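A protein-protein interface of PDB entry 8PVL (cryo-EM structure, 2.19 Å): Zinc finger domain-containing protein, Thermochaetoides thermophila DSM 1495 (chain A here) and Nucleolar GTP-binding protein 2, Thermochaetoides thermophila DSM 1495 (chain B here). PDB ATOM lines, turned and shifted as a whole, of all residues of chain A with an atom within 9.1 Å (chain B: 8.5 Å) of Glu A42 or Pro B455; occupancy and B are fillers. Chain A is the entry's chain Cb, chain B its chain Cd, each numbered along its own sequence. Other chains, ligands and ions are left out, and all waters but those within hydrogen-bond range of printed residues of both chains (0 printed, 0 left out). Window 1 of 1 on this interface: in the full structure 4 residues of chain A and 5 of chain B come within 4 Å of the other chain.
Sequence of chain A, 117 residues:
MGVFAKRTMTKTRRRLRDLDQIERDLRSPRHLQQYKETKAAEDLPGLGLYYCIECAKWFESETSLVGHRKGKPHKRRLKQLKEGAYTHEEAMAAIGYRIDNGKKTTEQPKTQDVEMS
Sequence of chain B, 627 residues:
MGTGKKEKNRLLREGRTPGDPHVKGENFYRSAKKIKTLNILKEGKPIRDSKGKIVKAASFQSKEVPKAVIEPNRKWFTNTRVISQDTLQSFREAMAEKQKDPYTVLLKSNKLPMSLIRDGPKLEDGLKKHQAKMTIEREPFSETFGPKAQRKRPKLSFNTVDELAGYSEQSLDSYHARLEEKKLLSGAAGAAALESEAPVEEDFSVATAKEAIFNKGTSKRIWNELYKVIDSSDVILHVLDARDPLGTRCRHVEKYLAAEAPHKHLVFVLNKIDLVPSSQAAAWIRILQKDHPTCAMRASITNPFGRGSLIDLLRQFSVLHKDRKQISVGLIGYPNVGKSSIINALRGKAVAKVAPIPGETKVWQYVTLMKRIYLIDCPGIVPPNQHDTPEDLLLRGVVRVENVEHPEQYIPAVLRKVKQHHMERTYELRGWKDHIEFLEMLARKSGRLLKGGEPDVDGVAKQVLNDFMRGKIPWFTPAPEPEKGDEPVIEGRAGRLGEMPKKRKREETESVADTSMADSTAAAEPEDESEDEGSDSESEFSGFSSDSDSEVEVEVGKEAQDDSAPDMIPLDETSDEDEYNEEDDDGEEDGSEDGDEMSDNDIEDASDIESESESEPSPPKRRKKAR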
ATOM      1  N   LYS A  36      10.488   4.342  19.483  1.00  0.00           N
ATOM      2  CA  LYS A  36       9.686   5.529  19.754  1.00  0.00           C
ATOM      3  C   LYS A  36       8.711   5.823  18.619  1.00  0.00           C
ATOM      4  O   LYS A  36       7.666   6.443  18.850  1.00  0.00           O
ATOM      5  CB  LYS A  36      10.598   6.726  20.009  1.00  0.00           C
ATOM      6  CG  LYS A  36      11.335   6.643  21.330  1.00  0.00           C
ATOM      7  CD  LYS A  36      12.024   7.946  21.665  1.00  0.00           C
ATOM      8  CE  LYS A  36      12.556   7.923  23.083  1.00  0.00           C
ATOM      9  NZ  LYS A  36      13.181   9.215  23.469  1.00  0.00           N
ATOM     10  N   LYS A  39       5.301   4.376  19.084  1.00  0.00           N
ATOM     11  CA  LYS A  39       4.461   5.031  20.078  1.00  0.00           C
ATOM     12  C   LYS A  39       3.856   6.305  19.496  1.00  0.00           C
ATOM     13  O   LYS A  39       4.219   6.756  18.407  1.00  0.00           O
ATOM     14  CB  LYS A  39       5.257   5.363  21.350  1.00  0.00           C
ATOM     15  CG  LYS A  39       5.243   4.307  22.466  1.00  0.00           C
ATOM     16  CD  LYS A  39       5.521   2.894  21.982  1.00  0.00           C
ATOM     17  CE  LYS A  39       5.806   1.957  23.145  1.00  0.00           C
ATOM     18  NZ  LYS A  39       4.626   1.784  24.034  1.00  0.00           N
ATOM     19  N   ALA A  40       2.920   6.886  20.243  1.00  0.00           N
ATOM     20  CA  ALA A  40       2.297   8.158  19.894  1.00  0.00           C
ATOM     21  C   ALA A  40       2.661   9.187  20.957  1.00  0.00           C
ATOM     22  O   ALA A  40       2.368   8.988  22.140  1.00  0.00           O
ATOM     23  CB  ALA A  40       0.780   8.015  19.776  1.00  0.00           C
ATOM     24  N   ALA A  41       3.278  10.290  20.526  1.00  0.00           N
ATOM     25  CA  ALA A  41       3.869  11.240  21.464  1.00  0.00           C
ATOM     26  C   ALA A  41       2.816  12.020  22.239  1.00  0.00           C
ATOM     27  O   ALA A  41       3.058  12.408  23.388  1.00  0.00           O
ATOM     28  CB  ALA A  41       4.795  12.201  20.722  1.00  0.00           C
ATOM     29  N   GLU A  42       1.655  12.269  21.631  1.00  0.00           N
ATOM     30  CA  GLU A  42       0.597  13.013  22.302  1.00  0.00           C
ATOM     31  C   GLU A  42       0.007  12.249  23.480  1.00  0.00           C
ATOM     32  O   GLU A  42      -0.436  12.876  24.449  1.00  0.00           O
ATOM     33  CB  GLU A  42      -0.523  13.391  21.317  1.00  0.00           C
ATOM     34  CG  GLU A  42      -0.996  12.314  20.314  1.00  0.00           C
ATOM     35  CD  GLU A  42      -0.065  12.084  19.122  1.00  0.00           C
ATOM     36  OE1 GLU A  42       1.074  12.596  19.124  1.00  0.00           O
ATOM     37  OE2 GLU A  42      -0.485  11.387  18.175  1.00  0.00           O
ATOM     38  N   ASP A  43      -0.009  10.919  23.424  1.00  0.00           N
ATOM     39  CA  ASP A  43      -0.487  10.108  24.536  1.00  0.00           C
ATOM     40  C   ASP A  43       0.586   9.831  25.581  1.00  0.00           C
ATOM     41  O   ASP A  43       0.255   9.345  26.667  1.00  0.00           O
ATOM     42  CB  ASP A  43      -1.040   8.775  24.020  1.00  0.00           C
ATOM     43  CG  ASP A  43      -1.917   8.942  22.797  1.00  0.00           C
ATOM     44  OD1 ASP A  43      -2.286  10.092  22.483  1.00  0.00           O
ATOM     45  OD2 ASP A  43      -2.231   7.923  22.145  1.00  0.00           O
ATOM     46  N   LEU A  44       1.850  10.130  25.285  1.00  0.00           N
ATOM     47  CA  LEU A  44       2.955   9.843  26.184  1.00  0.00           C
ATOM     48  C   LEU A  44       2.954  10.795  27.379  1.00  0.00           C
ATOM     49  O   LEU A  44       2.485  11.931  27.275  1.00  0.00           O
ATOM     50  CB  LEU A  44       4.285   9.949  25.447  1.00  0.00           C
ATOM     51  CG  LEU A  44       4.629   8.791  24.509  1.00  0.00           C
ATOM     52  CD1 LEU A  44       5.914   9.078  23.753  1.00  0.00           C
ATOM     53  CD2 LEU A  44       4.725   7.483  25.273  1.00  0.00           C
ATOM     54  N   PRO A  45       3.451  10.340  28.531  1.00  0.00           N
ATOM     55  CA  PRO A  45       3.631  11.251  29.670  1.00  0.00           C
ATOM     56  C   PRO A  45       4.656  12.329  29.349  1.00  0.00           C
ATOM     57  O   PRO A  45       5.745  12.043  28.847  1.00  0.00           O
ATOM     58  CB  PRO A  45       4.122  10.328  30.793  1.00  0.00           C
ATOM     59  CG  PRO A  45       3.783   8.948  30.362  1.00  0.00           C
ATOM     60  CD  PRO A  45       3.757   8.941  28.876  1.00  0.00           C
ATOM     61  N   GLY A  46       4.299  13.576  29.649  1.00  0.00           N
ATOM     62  CA  GLY A  46       5.192  14.694  29.394  1.00  0.00           C
ATOM     63  C   GLY A  46       5.467  14.945  27.929  1.00  0.00           C
ATOM     64  O   GLY A  46       6.512  15.514  27.593  1.00  0.00           O
ATOM     65  N   LEU A  47       4.560  14.511  27.046  1.00  0.00           N
ATOM     66  CA  LEU A  47       4.687  14.625  25.588  1.00  0.00           C
ATOM     67  C   LEU A  47       5.931  13.913  25.061  1.00  0.00           C
ATOM     68  O   LEU A  47       6.478  14.285  24.020  1.00  0.00           O
ATOM     69  CB  LEU A  47       4.671  16.088  25.109  1.00  0.00           C
ATOM     70  CG  LEU A  47       3.401  16.958  25.068  1.00  0.00           C
ATOM     71  CD1 LEU A  47       2.496  16.517  23.924  1.00  0.00           C
ATOM     72  CD2 LEU A  47       2.623  17.041  26.381  1.00  0.00           C
ATOM     73  N   GLY A  48       6.385  12.879  25.769  1.00  0.00           N
ATOM     74  CA  GLY A  48       7.539  12.115  25.342  1.00  0.00           C
ATOM     75  C   GLY A  48       8.864  12.834  25.420  1.00  0.00           C
ATOM     76  O   GLY A  48       9.817  12.417  24.754  1.00  0.00           O
ATOM     77  N   LEU A  49       8.963  13.902  26.211  1.00  0.00           N
ATOM     78  CA  LEU A  49      10.206  14.661  26.282  1.00  0.00           C
ATOM     79  C   LEU A  49      11.162  14.110  27.330  1.00  0.00           C
ATOM     80  O   LEU A  49      12.380  14.268  27.194  1.00  0.00           O
ATOM     81  CB  LEU A  49       9.909  16.131  26.576  1.00  0.00           C
ATOM     82  CG  LEU A  49       9.035  16.861  25.555  1.00  0.00           C
ATOM     83  CD1 LEU A  49       8.803  18.299  25.982  1.00  0.00           C
ATOM     84  CD2 LEU A  49       9.673  16.805  24.181  1.00  0.00           C
ATOM     85  N   TRP A  58       8.770   6.568  30.418  1.00  0.00           N
ATOM     86  CA  TRP A  58       8.458   7.975  30.202  1.00  0.00           C
ATOM     87  C   TRP A  58       7.993   8.613  31.505  1.00  0.00           C
ATOM     88  O   TRP A  58       7.299   7.980  32.304  1.00  0.00           O
ATOM     89  CB  TRP A  58       7.378   8.137  29.133  1.00  0.00           C
ATOM     90  CG  TRP A  58       7.899   8.090  27.735  1.00  0.00           C
ATOM     91  CD1 TRP A  58       8.477   9.112  27.043  1.00  0.00           C
ATOM     92  CD2 TRP A  58       7.886   6.964  26.850  1.00  0.00           C
ATOM     93  NE1 TRP A  58       8.826   8.694  25.785  1.00  0.00           N
ATOM     94  CE2 TRP A  58       8.472   7.379  25.640  1.00  0.00           C
ATOM     95  CE3 TRP A  58       7.435   5.646  26.965  1.00  0.00           C
ATOM     96  CZ2 TRP A  58       8.625   6.523  24.554  1.00  0.00           C
ATOM     97  CZ3 TRP A  58       7.585   4.799  25.884  1.00  0.00           C
ATOM     98  CH2 TRP A  58       8.175   5.240  24.694  1.00  0.00           C
ATOM     99  N   GLU B 408     -15.454  13.892  20.067  1.00  0.00           N
ATOM    100  CA  GLU B 408     -14.479  14.870  19.603  1.00  0.00           C
ATOM    101  C   GLU B 408     -14.757  15.353  18.185  1.00  0.00           C
ATOM    102  O   GLU B 408     -14.289  16.433  17.813  1.00  0.00           O
ATOM    103  CB  GLU B 408     -13.067  14.281  19.674  1.00  0.00           C
ATOM    104  CG  GLU B 408     -12.679  13.712  21.032  1.00  0.00           C
ATOM    105  CD  GLU B 408     -12.970  12.225  21.160  1.00  0.00           C
ATOM    106  OE1 GLU B 408     -13.882  11.728  20.466  1.00  0.00           O
ATOM    107  OE2 GLU B 408     -12.283  11.550  21.954  1.00  0.00           O
ATOM    108  N   ILE B 436      -8.325  19.328  18.259  1.00  0.00           N
ATOM    109  CA  ILE B 436      -7.624  18.291  19.013  1.00  0.00           C
ATOM    110  C   ILE B 436      -6.662  18.919  20.017  1.00  0.00           C
ATOM    111  O   ILE B 436      -6.632  18.533  21.193  1.00  0.00           O
ATOM    112  CB  ILE B 436      -6.901  17.333  18.051  1.00  0.00           C
ATOM    113  CG1 ILE B 436      -7.920  16.508  17.265  1.00  0.00           C
ATOM    114  CG2 ILE B 436      -5.953  16.420  18.806  1.00  0.00           C
ATOM    115  CD1 ILE B 436      -8.803  15.640  18.135  1.00  0.00           C
ATOM    116  N   GLU B 437      -5.889  19.916  19.578  1.00  0.00           N
ATOM    117  CA  GLU B 437      -4.990  20.599  20.501  1.00  0.00           C
ATOM    118  C   GLU B 437      -5.759  21.417  21.530  1.00  0.00           C
ATOM    119  O   GLU B 437      -5.310  21.533  22.676  1.00  0.00           O
ATOM    120  CB  GLU B 437      -4.012  21.499  19.748  1.00  0.00           C
ATOM    121  CG  GLU B 437      -2.863  21.987  20.619  1.00  0.00           C
ATOM    122  CD  GLU B 437      -2.027  23.055  19.956  1.00  0.00           C
ATOM    123  OE1 GLU B 437      -2.237  23.309  18.756  1.00  0.00           O
ATOM    124  OE2 GLU B 437      -1.161  23.644  20.636  1.00  0.00           O
ATOM    125  N   PHE B 438      -6.912  21.981  21.149  1.00  0.00           N
ATOM    126  CA  PHE B 438      -7.750  22.673  22.128  1.00  0.00           C
ATOM    127  C   PHE B 438      -8.208  21.724  23.229  1.00  0.00           C
ATOM    128  O   PHE B 438      -8.131  22.051  24.422  1.00  0.00           O
ATOM    129  CB  PHE B 438      -8.959  23.310  21.439  1.00  0.00           C
ATOM    130  CG  PHE B 438     -10.062  23.676  22.388  1.00  0.00           C
ATOM    131  CD1 PHE B 438      -9.947  24.793  23.196  1.00  0.00           C
ATOM    132  CD2 PHE B 438     -11.210  22.901  22.479  1.00  0.00           C
ATOM    133  CE1 PHE B 438     -10.949  25.131  24.079  1.00  0.00           C
ATOM    134  CE2 PHE B 438     -12.214  23.233  23.364  1.00  0.00           C
ATOM    135  CZ  PHE B 438     -12.083  24.349  24.162  1.00  0.00           C
ATOM    136  N   LEU B 439      -8.686  20.538  22.843  1.00  0.00           N
ATOM    137  CA  LEU B 439      -9.145  19.558  23.821  1.00  0.00           C
ATOM    138  C   LEU B 439      -7.996  19.062  24.691  1.00  0.00           C
ATOM    139  O   LEU B 439      -8.167  18.877  25.899  1.00  0.00           O
ATOM    140  CB  LEU B 439      -9.833  18.390  23.114  1.00  0.00           C
ATOM    141  CG  LEU B 439     -11.172  18.701  22.437  1.00  0.00           C
ATOM    142  CD1 LEU B 439     -11.650  17.524  21.605  1.00  0.00           C
ATOM    143  CD2 LEU B 439     -12.227  19.112  23.447  1.00  0.00           C
ATOM    144  N   GLU B 440      -6.815  18.859  24.097  1.00  0.00           N
ATOM    145  CA  GLU B 440      -5.665  18.400  24.872  1.00  0.00           C
ATOM    146  C   GLU B 440      -5.197  19.454  25.870  1.00  0.00           C
ATOM    147  O   GLU B 440      -4.868  19.123  27.019  1.00  0.00           O
ATOM    148  CB  GLU B 440      -4.525  18.005  23.935  1.00  0.00           C
ATOM    149  CG  GLU B 440      -4.767  16.707  23.191  1.00  0.00           C
ATOM    150  CD  GLU B 440      -3.876  16.558  21.975  1.00  0.00           C
ATOM    151  OE1 GLU B 440      -3.148  17.518  21.649  1.00  0.00           O
ATOM    152  OE2 GLU B 440      -3.906  15.483  21.342  1.00  0.00           O
ATOM    153  N   MET B 441      -5.162  20.726  25.457  1.00  0.00           N
ATOM    154  CA  MET B 441      -4.782  21.793  26.377  1.00  0.00           C
ATOM    155  C   MET B 441      -5.797  21.946  27.502  1.00  0.00           C
ATOM    156  O   MET B 441      -5.413  22.141  28.660  1.00  0.00           O
ATOM    157  CB  MET B 441      -4.614  23.115  25.629  1.00  0.00           C
ATOM    158  CG  MET B 441      -3.370  23.204  24.765  1.00  0.00           C
ATOM    159  SD  MET B 441      -3.608  24.279  23.340  1.00  0.00           S
ATOM    160  CE  MET B 441      -3.916  25.847  24.145  1.00  0.00           C
ATOM    161  N   LEU B 442      -7.093  21.850  27.185  1.00  0.00           N
ATOM    162  CA  LEU B 442      -8.110  21.917  28.230  1.00  0.00           C
ATOM    163  C   LEU B 442      -7.995  20.741  29.194  1.00  0.00           C
ATOM    164  O   LEU B 442      -8.163  20.909  30.407  1.00  0.00           O
ATOM    165  CB  LEU B 442      -9.506  21.968  27.608  1.00  0.00           C
ATOM    166  CG  LEU B 442     -10.682  22.221  28.554  1.00  0.00           C
ATOM    167  CD1 LEU B 442     -10.372  23.328  29.551  1.00  0.00           C
ATOM    168  CD2 LEU B 442     -11.935  22.558  27.765  1.00  0.00           C
ATOM    169  N   ALA B 443      -7.704  19.546  28.671  1.00  0.00           N
ATOM    170  CA  ALA B 443      -7.567  18.368  29.522  1.00  0.00           C
ATOM    171  C   ALA B 443      -6.369  18.484  30.454  1.00  0.00           C
ATOM    172  O   ALA B 443      -6.472  18.162  31.644  1.00  0.00           O
ATOM    173  CB  ALA B 443      -7.454  17.113  28.662  1.00  0.00           C
ATOM    174  N   ARG B 444      -5.228  18.945  29.937  1.00  0.00           N
ATOM    175  CA  ARG B 444      -4.058  19.108  30.794  1.00  0.00           C
ATOM    176  C   ARG B 444      -4.235  20.253  31.782  1.00  0.00           C
ATOM    177  O   ARG B 444      -3.679  20.206  32.885  1.00  0.00           O
ATOM    178  CB  ARG B 444      -2.803  19.323  29.951  1.00  0.00           C
ATOM    179  CG  ARG B 444      -2.443  18.136  29.085  1.00  0.00           C
ATOM    180  CD  ARG B 444      -1.004  18.206  28.618  1.00  0.00           C
ATOM    181  NE  ARG B 444      -0.788  17.362  27.450  1.00  0.00           N
ATOM    182  CZ  ARG B 444      -0.867  17.787  26.198  1.00  0.00           C
ATOM    183  NH1 ARG B 444      -1.126  19.053  25.913  1.00  0.00           N
ATOM    184  NH2 ARG B 444      -0.685  16.921  25.205  1.00  0.00           N
ATOM    185  N   LYS B 445      -5.003  21.281  31.417  1.00  0.00           N
ATOM    186  CA  LYS B 445      -5.259  22.373  32.349  1.00  0.00           C
ATOM    187  C   LYS B 445      -6.185  21.937  33.478  1.00  0.00           C
ATOM    188  O   LYS B 445      -5.926  22.234  34.650  1.00  0.00           O
ATOM    189  CB  LYS B 445      -5.849  23.567  31.601  1.00  0.00           C
ATOM    190  CG  LYS B 445      -6.291  24.700  32.501  1.00  0.00           C
ATOM    191  CD  LYS B 445      -6.612  25.948  31.706  1.00  0.00           C
ATOM    192  CE  LYS B 445      -7.246  27.005  32.590  1.00  0.00           C
ATOM    193  NZ  LYS B 445      -6.423  28.240  32.651  1.00  0.00           N
ATOM    194  N   GLY B 447      -6.842  18.849  34.444  1.00  0.00           N
ATOM    195  CA  GLY B 447      -6.466  17.613  35.094  1.00  0.00           C
ATOM    196  C   GLY B 447      -7.254  16.398  34.673  1.00  0.00           C
ATOM    197  O   GLY B 447      -7.291  15.412  35.414  1.00  0.00           O
ATOM    198  N   ARG B 448      -7.894  16.432  33.504  1.00  0.00           N
ATOM    199  CA  ARG B 448      -8.644  15.284  32.999  1.00  0.00           C
ATOM    200  C   ARG B 448      -7.673  14.353  32.282  1.00  0.00           C
ATOM    201  O   ARG B 448      -7.560  14.331  31.057  1.00  0.00           O
ATOM    202  CB  ARG B 448      -9.780  15.737  32.090  1.00  0.00           C
ATOM    203  CG  ARG B 448     -10.748  16.730  32.727  1.00  0.00           C
ATOM    204  CD  ARG B 448     -11.939  16.063  33.425  1.00  0.00           C
ATOM    205  NE  ARG B 448     -11.545  15.118  34.461  1.00  0.00           N
ATOM    206  CZ  ARG B 448     -11.315  15.443  35.725  1.00  0.00           C
ATOM    207  NH1 ARG B 448     -11.443  16.686  36.153  1.00  0.00           N
ATOM    208  NH2 ARG B 448     -10.945  14.494  36.581  1.00  0.00           N
ATOM    209  N   LEU B 449      -6.961  13.567  33.080  1.00  0.00           N
ATOM    210  CA  LEU B 449      -5.904  12.696  32.593  1.00  0.00           C
ATOM    211  C   LEU B 449      -6.293  11.238  32.783  1.00  0.00           C
ATOM    212  O   LEU B 449      -6.905  10.873  33.789  1.00  0.00           O
ATOM    213  CB  LEU B 449      -4.590  12.978  33.320  1.00  0.00           C
ATOM    214  CG  LEU B 449      -4.221  14.452  33.468  1.00  0.00           C
ATOM    215  CD1 LEU B 449      -3.060  14.622  34.432  1.00  0.00           C
ATOM    216  CD2 LEU B 449      -3.894  15.052  32.111  1.00  0.00           C
ATOM    217  N   LEU B 450      -5.942  10.414  31.804  1.00  0.00           N
ATOM    218  CA  LEU B 450      -6.056   8.971  31.927  1.00  0.00           C
ATOM    219  C   LEU B 450      -4.777   8.435  32.570  1.00  0.00           C
ATOM    220  O   LEU B 450      -3.974   9.192  33.122  1.00  0.00           O
ATOM    221  CB  LEU B 450      -6.340   8.344  30.565  1.00  0.00           C
ATOM    222  CG  LEU B 450      -7.562   8.892  29.826  1.00  0.00           C
ATOM    223  CD1 LEU B 450      -7.706   8.243  28.462  1.00  0.00           C
ATOM    224  CD2 LEU B 450      -8.825   8.700  30.650  1.00  0.00           C
ATOM    225  N   LYS B 451      -4.583   7.119  32.523  1.00  0.00           N
ATOM    226  CA  LYS B 451      -3.394   6.513  33.107  1.00  0.00           C
ATOM    227  C   LYS B 451      -2.148   6.925  32.334  1.00  0.00           C
ATOM    228  O   LYS B 451      -2.133   6.906  31.100  1.00  0.00           O
ATOM    229  CB  LYS B 451      -3.529   4.992  33.127  1.00  0.00           C
ATOM    230  CG  LYS B 451      -4.575   4.488  34.104  1.00  0.00           C
ATOM    231  CD  LYS B 451      -4.267   4.951  35.515  1.00  0.00           C
ATOM    232  CE  LYS B 451      -5.273   4.404  36.513  1.00  0.00           C
ATOM    233  NZ  LYS B 451      -5.024   4.931  37.883  1.00  0.00           N
ATOM    234  N   GLY B 452      -1.102   7.298  33.065  1.00  0.00           N
ATOM    235  CA  GLY B 452       0.085   7.848  32.451  1.00  0.00           C
ATOM    236  C   GLY B 452      -0.016   9.304  32.061  1.00  0.00           C
ATOM    237  O   GLY B 452       0.832   9.786  31.305  1.00  0.00           O
ATOM    238  N   GLY B 453      -1.030  10.022  32.537  1.00  0.00           N
ATOM    239  CA  GLY B 453      -1.170  11.416  32.179  1.00  0.00           C
ATOM    240  C   GLY B 453      -1.669  11.676  30.777  1.00  0.00           C
ATOM    241  O   GLY B 453      -1.563  12.810  30.303  1.00  0.00           O
ATOM    242  N   GLU B 454      -2.190  10.663  30.094  1.00  0.00           N
ATOM    243  CA  GLU B 454      -2.747  10.865  28.763  1.00  0.00           C
ATOM    244  C   GLU B 454      -4.029  11.687  28.859  1.00  0.00           C
ATOM    245  O   GLU B 454      -4.903  11.364  29.672  1.00  0.00           O
ATOM    246  CB  GLU B 454      -3.025   9.524  28.088  1.00  0.00           C
ATOM    247  CG  GLU B 454      -3.754   9.643  26.761  1.00  0.00           C
ATOM    248  CD  GLU B 454      -4.403   8.346  26.330  1.00  0.00           C
ATOM    249  OE1 GLU B 454      -4.301   7.350  27.076  1.00  0.00           O
ATOM    250  OE2 GLU B 454      -5.017   8.322  25.243  1.00  0.00           O
ATOM    251  N   PRO B 455      -4.167  12.757  28.075  1.00  0.00           N
ATOM    252  CA  PRO B 455      -5.348  13.622  28.194  1.00  0.00           C
ATOM    253  C   PRO B 455      -6.628  12.930  27.746  1.00  0.00           C
ATOM    254  O   PRO B 455      -6.648  12.190  26.760  1.00  0.00           O
ATOM    255  CB  PRO B 455      -5.006  14.808  27.286  1.00  0.00           C
ATOM    256  CG  PRO B 455      -3.974  14.288  26.347  1.00  0.00           C
ATOM    257  CD  PRO B 455      -3.178  13.297  27.127  1.00  0.00           C
ATOM    258  N   ASP B 456      -7.709  13.189  28.485  1.00  0.00           N
ATOM    259  CA  ASP B 456      -9.009  12.565  28.228  1.00  0.00           C
ATOM    260  C   ASP B 456      -9.827  13.478  27.317  1.00  0.00           C
ATOM    261  O   ASP B 456     -10.727  14.208  27.746  1.00  0.00           O
ATOM    262  CB  ASP B 456      -9.735  12.276  29.535  1.00  0.00           C
ATOM    263  CG  ASP B 456     -10.952  11.395  29.344  1.00  0.00           C
ATOM    264  OD1 ASP B 456     -11.058  10.740  28.286  1.00  0.00           O
ATOM    265  OD2 ASP B 456     -11.807  11.356  30.252  1.00  0.00           O
ATOM    266  N   VAL B 457      -9.503  13.411  26.023  1.00  0.00           N
ATOM    267  CA  VAL B 457     -10.163  14.260  25.037  1.00  0.00           C
ATOM    268  C   VAL B 457     -11.634  13.893  24.895  1.00  0.00           C
ATOM    269  O   VAL B 457     -12.464  14.760  24.610  1.00  0.00           O
ATOM    270  CB  VAL B 457      -9.422  14.190  23.689  1.00  0.00           C
ATOM    271  CG1 VAL B 457      -8.089  14.909  23.788  1.00  0.00           C
ATOM    272  CG2 VAL B 457      -9.214  12.750  23.259  1.00  0.00           C
ATOM    273  N   ASP B 458     -11.984  12.623  25.126  1.00  0.00           N
ATOM    274  CA  ASP B 458     -13.379  12.190  25.072  1.00  0.00           C
ATOM    275  C   ASP B 458     -14.218  12.887  26.140  1.00  0.00           C
ATOM    276  O   ASP B 458     -15.254  13.501  25.842  1.00  0.00           O
ATOM    277  CB  ASP B 458     -13.439  10.672  25.255  1.00  0.00           C
ATOM    278  CG  ASP B 458     -14.568  10.031  24.484  1.00  0.00           C
ATOM    279  OD1 ASP B 458     -15.637   9.788  25.082  1.00  0.00           O
ATOM    280  OD2 ASP B 458     -14.369   9.737  23.287  1.00  0.00           O
ATOM    281  N   GLY B 459     -13.767  12.818  27.394  1.00  0.00           N
ATOM    282  CA  GLY B 459     -14.498  13.455  28.476  1.00  0.00           C
ATOM    283  C   GLY B 459     -14.498  14.966  28.375  1.00  0.00           C
ATOM    284  O   GLY B 459     -15.494  15.618  28.702  1.00  0.00           O
ATOM    285  N   VAL B 460     -13.388  15.545  27.911  1.00  0.00           N
ATOM    286  CA  VAL B 460     -13.330  16.996  27.762  1.00  0.00           C
ATOM    287  C   VAL B 460     -14.263  17.462  26.645  1.00  0.00           C
ATOM    288  O   VAL B 460     -14.934  18.492  26.774  1.00  0.00           O
ATOM    289  CB  VAL B 460     -11.872  17.441  27.550  1.00  0.00           C
ATOM    290  CG1 VAL B 460     -11.788  18.885  27.102  1.00  0.00           C
ATOM    291  CG2 VAL B 460     -11.109  17.273  28.843  1.00  0.00           C
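CB of Glu A42 touches OE2 of Glu B440, 3.98 Å away. Pro B455 touches Glu A42 (CD to O, 3.9 Å). Asp A43 touches Glu B454 (O to CB, 3.6 Å). Pro A45 touches Gly B452. NH2 of Arg B444 touches CD1 of Leu A47, at 3.5 Å.
Of chain B, only Glu B440 (3.98 Å) and Pro B455 (3.9 Å) come within 4 Å of Glu A42. Of the printed residues of chain A, Pro B455 touches Glu A42 (3.9 Å). Ala A41 touches none of the printed residues of chain B. Of the printed residues of chain A, Arg B444 touches Leu A47. Printed residues of chain A within 4 Å of Glu B440: Glu A42 (3.98 Å). Of the printed residues of chain B, Pro A45 touches Gly B452. Printed residues of chain A within 4 Å of Glu B454: Asp A43 (3.6 Å). Gly B459 touches none of the printed residues of chain A. The nearest residue of chain B that does not touch Glu A42 is Arg B444 (4.1 Å). The nearest residue of chain A that does not touch Pro B455 is Asp A43 (4.9 Å). The nearest printed residue of chain A that does not touch Glu B454 is Glu A42 (5.2 Å).
Of the 25 printed residues of chain B, 5 touch a printed residue of chain A. Printed residues of chain B that touch a printed residue of chain A: Glu B440, Arg B444, Gly B452, Glu B454 and Pro B455. Hydrophobic or aromatic side chains of chain B within 4 Å of the printed part of chain A: Pro B455. Of the 13 printed residues of chain A, 4 touch a printed residue of chain B. Printed residues of chain A that touch a printed residue of chain B: Glu A42, Asp A43, Pro A45 and Leu A47. Hydrophobic or aromatic side chains of chain A within 4 Å of the printed part of chain B: Pro A45 and Leu A47.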
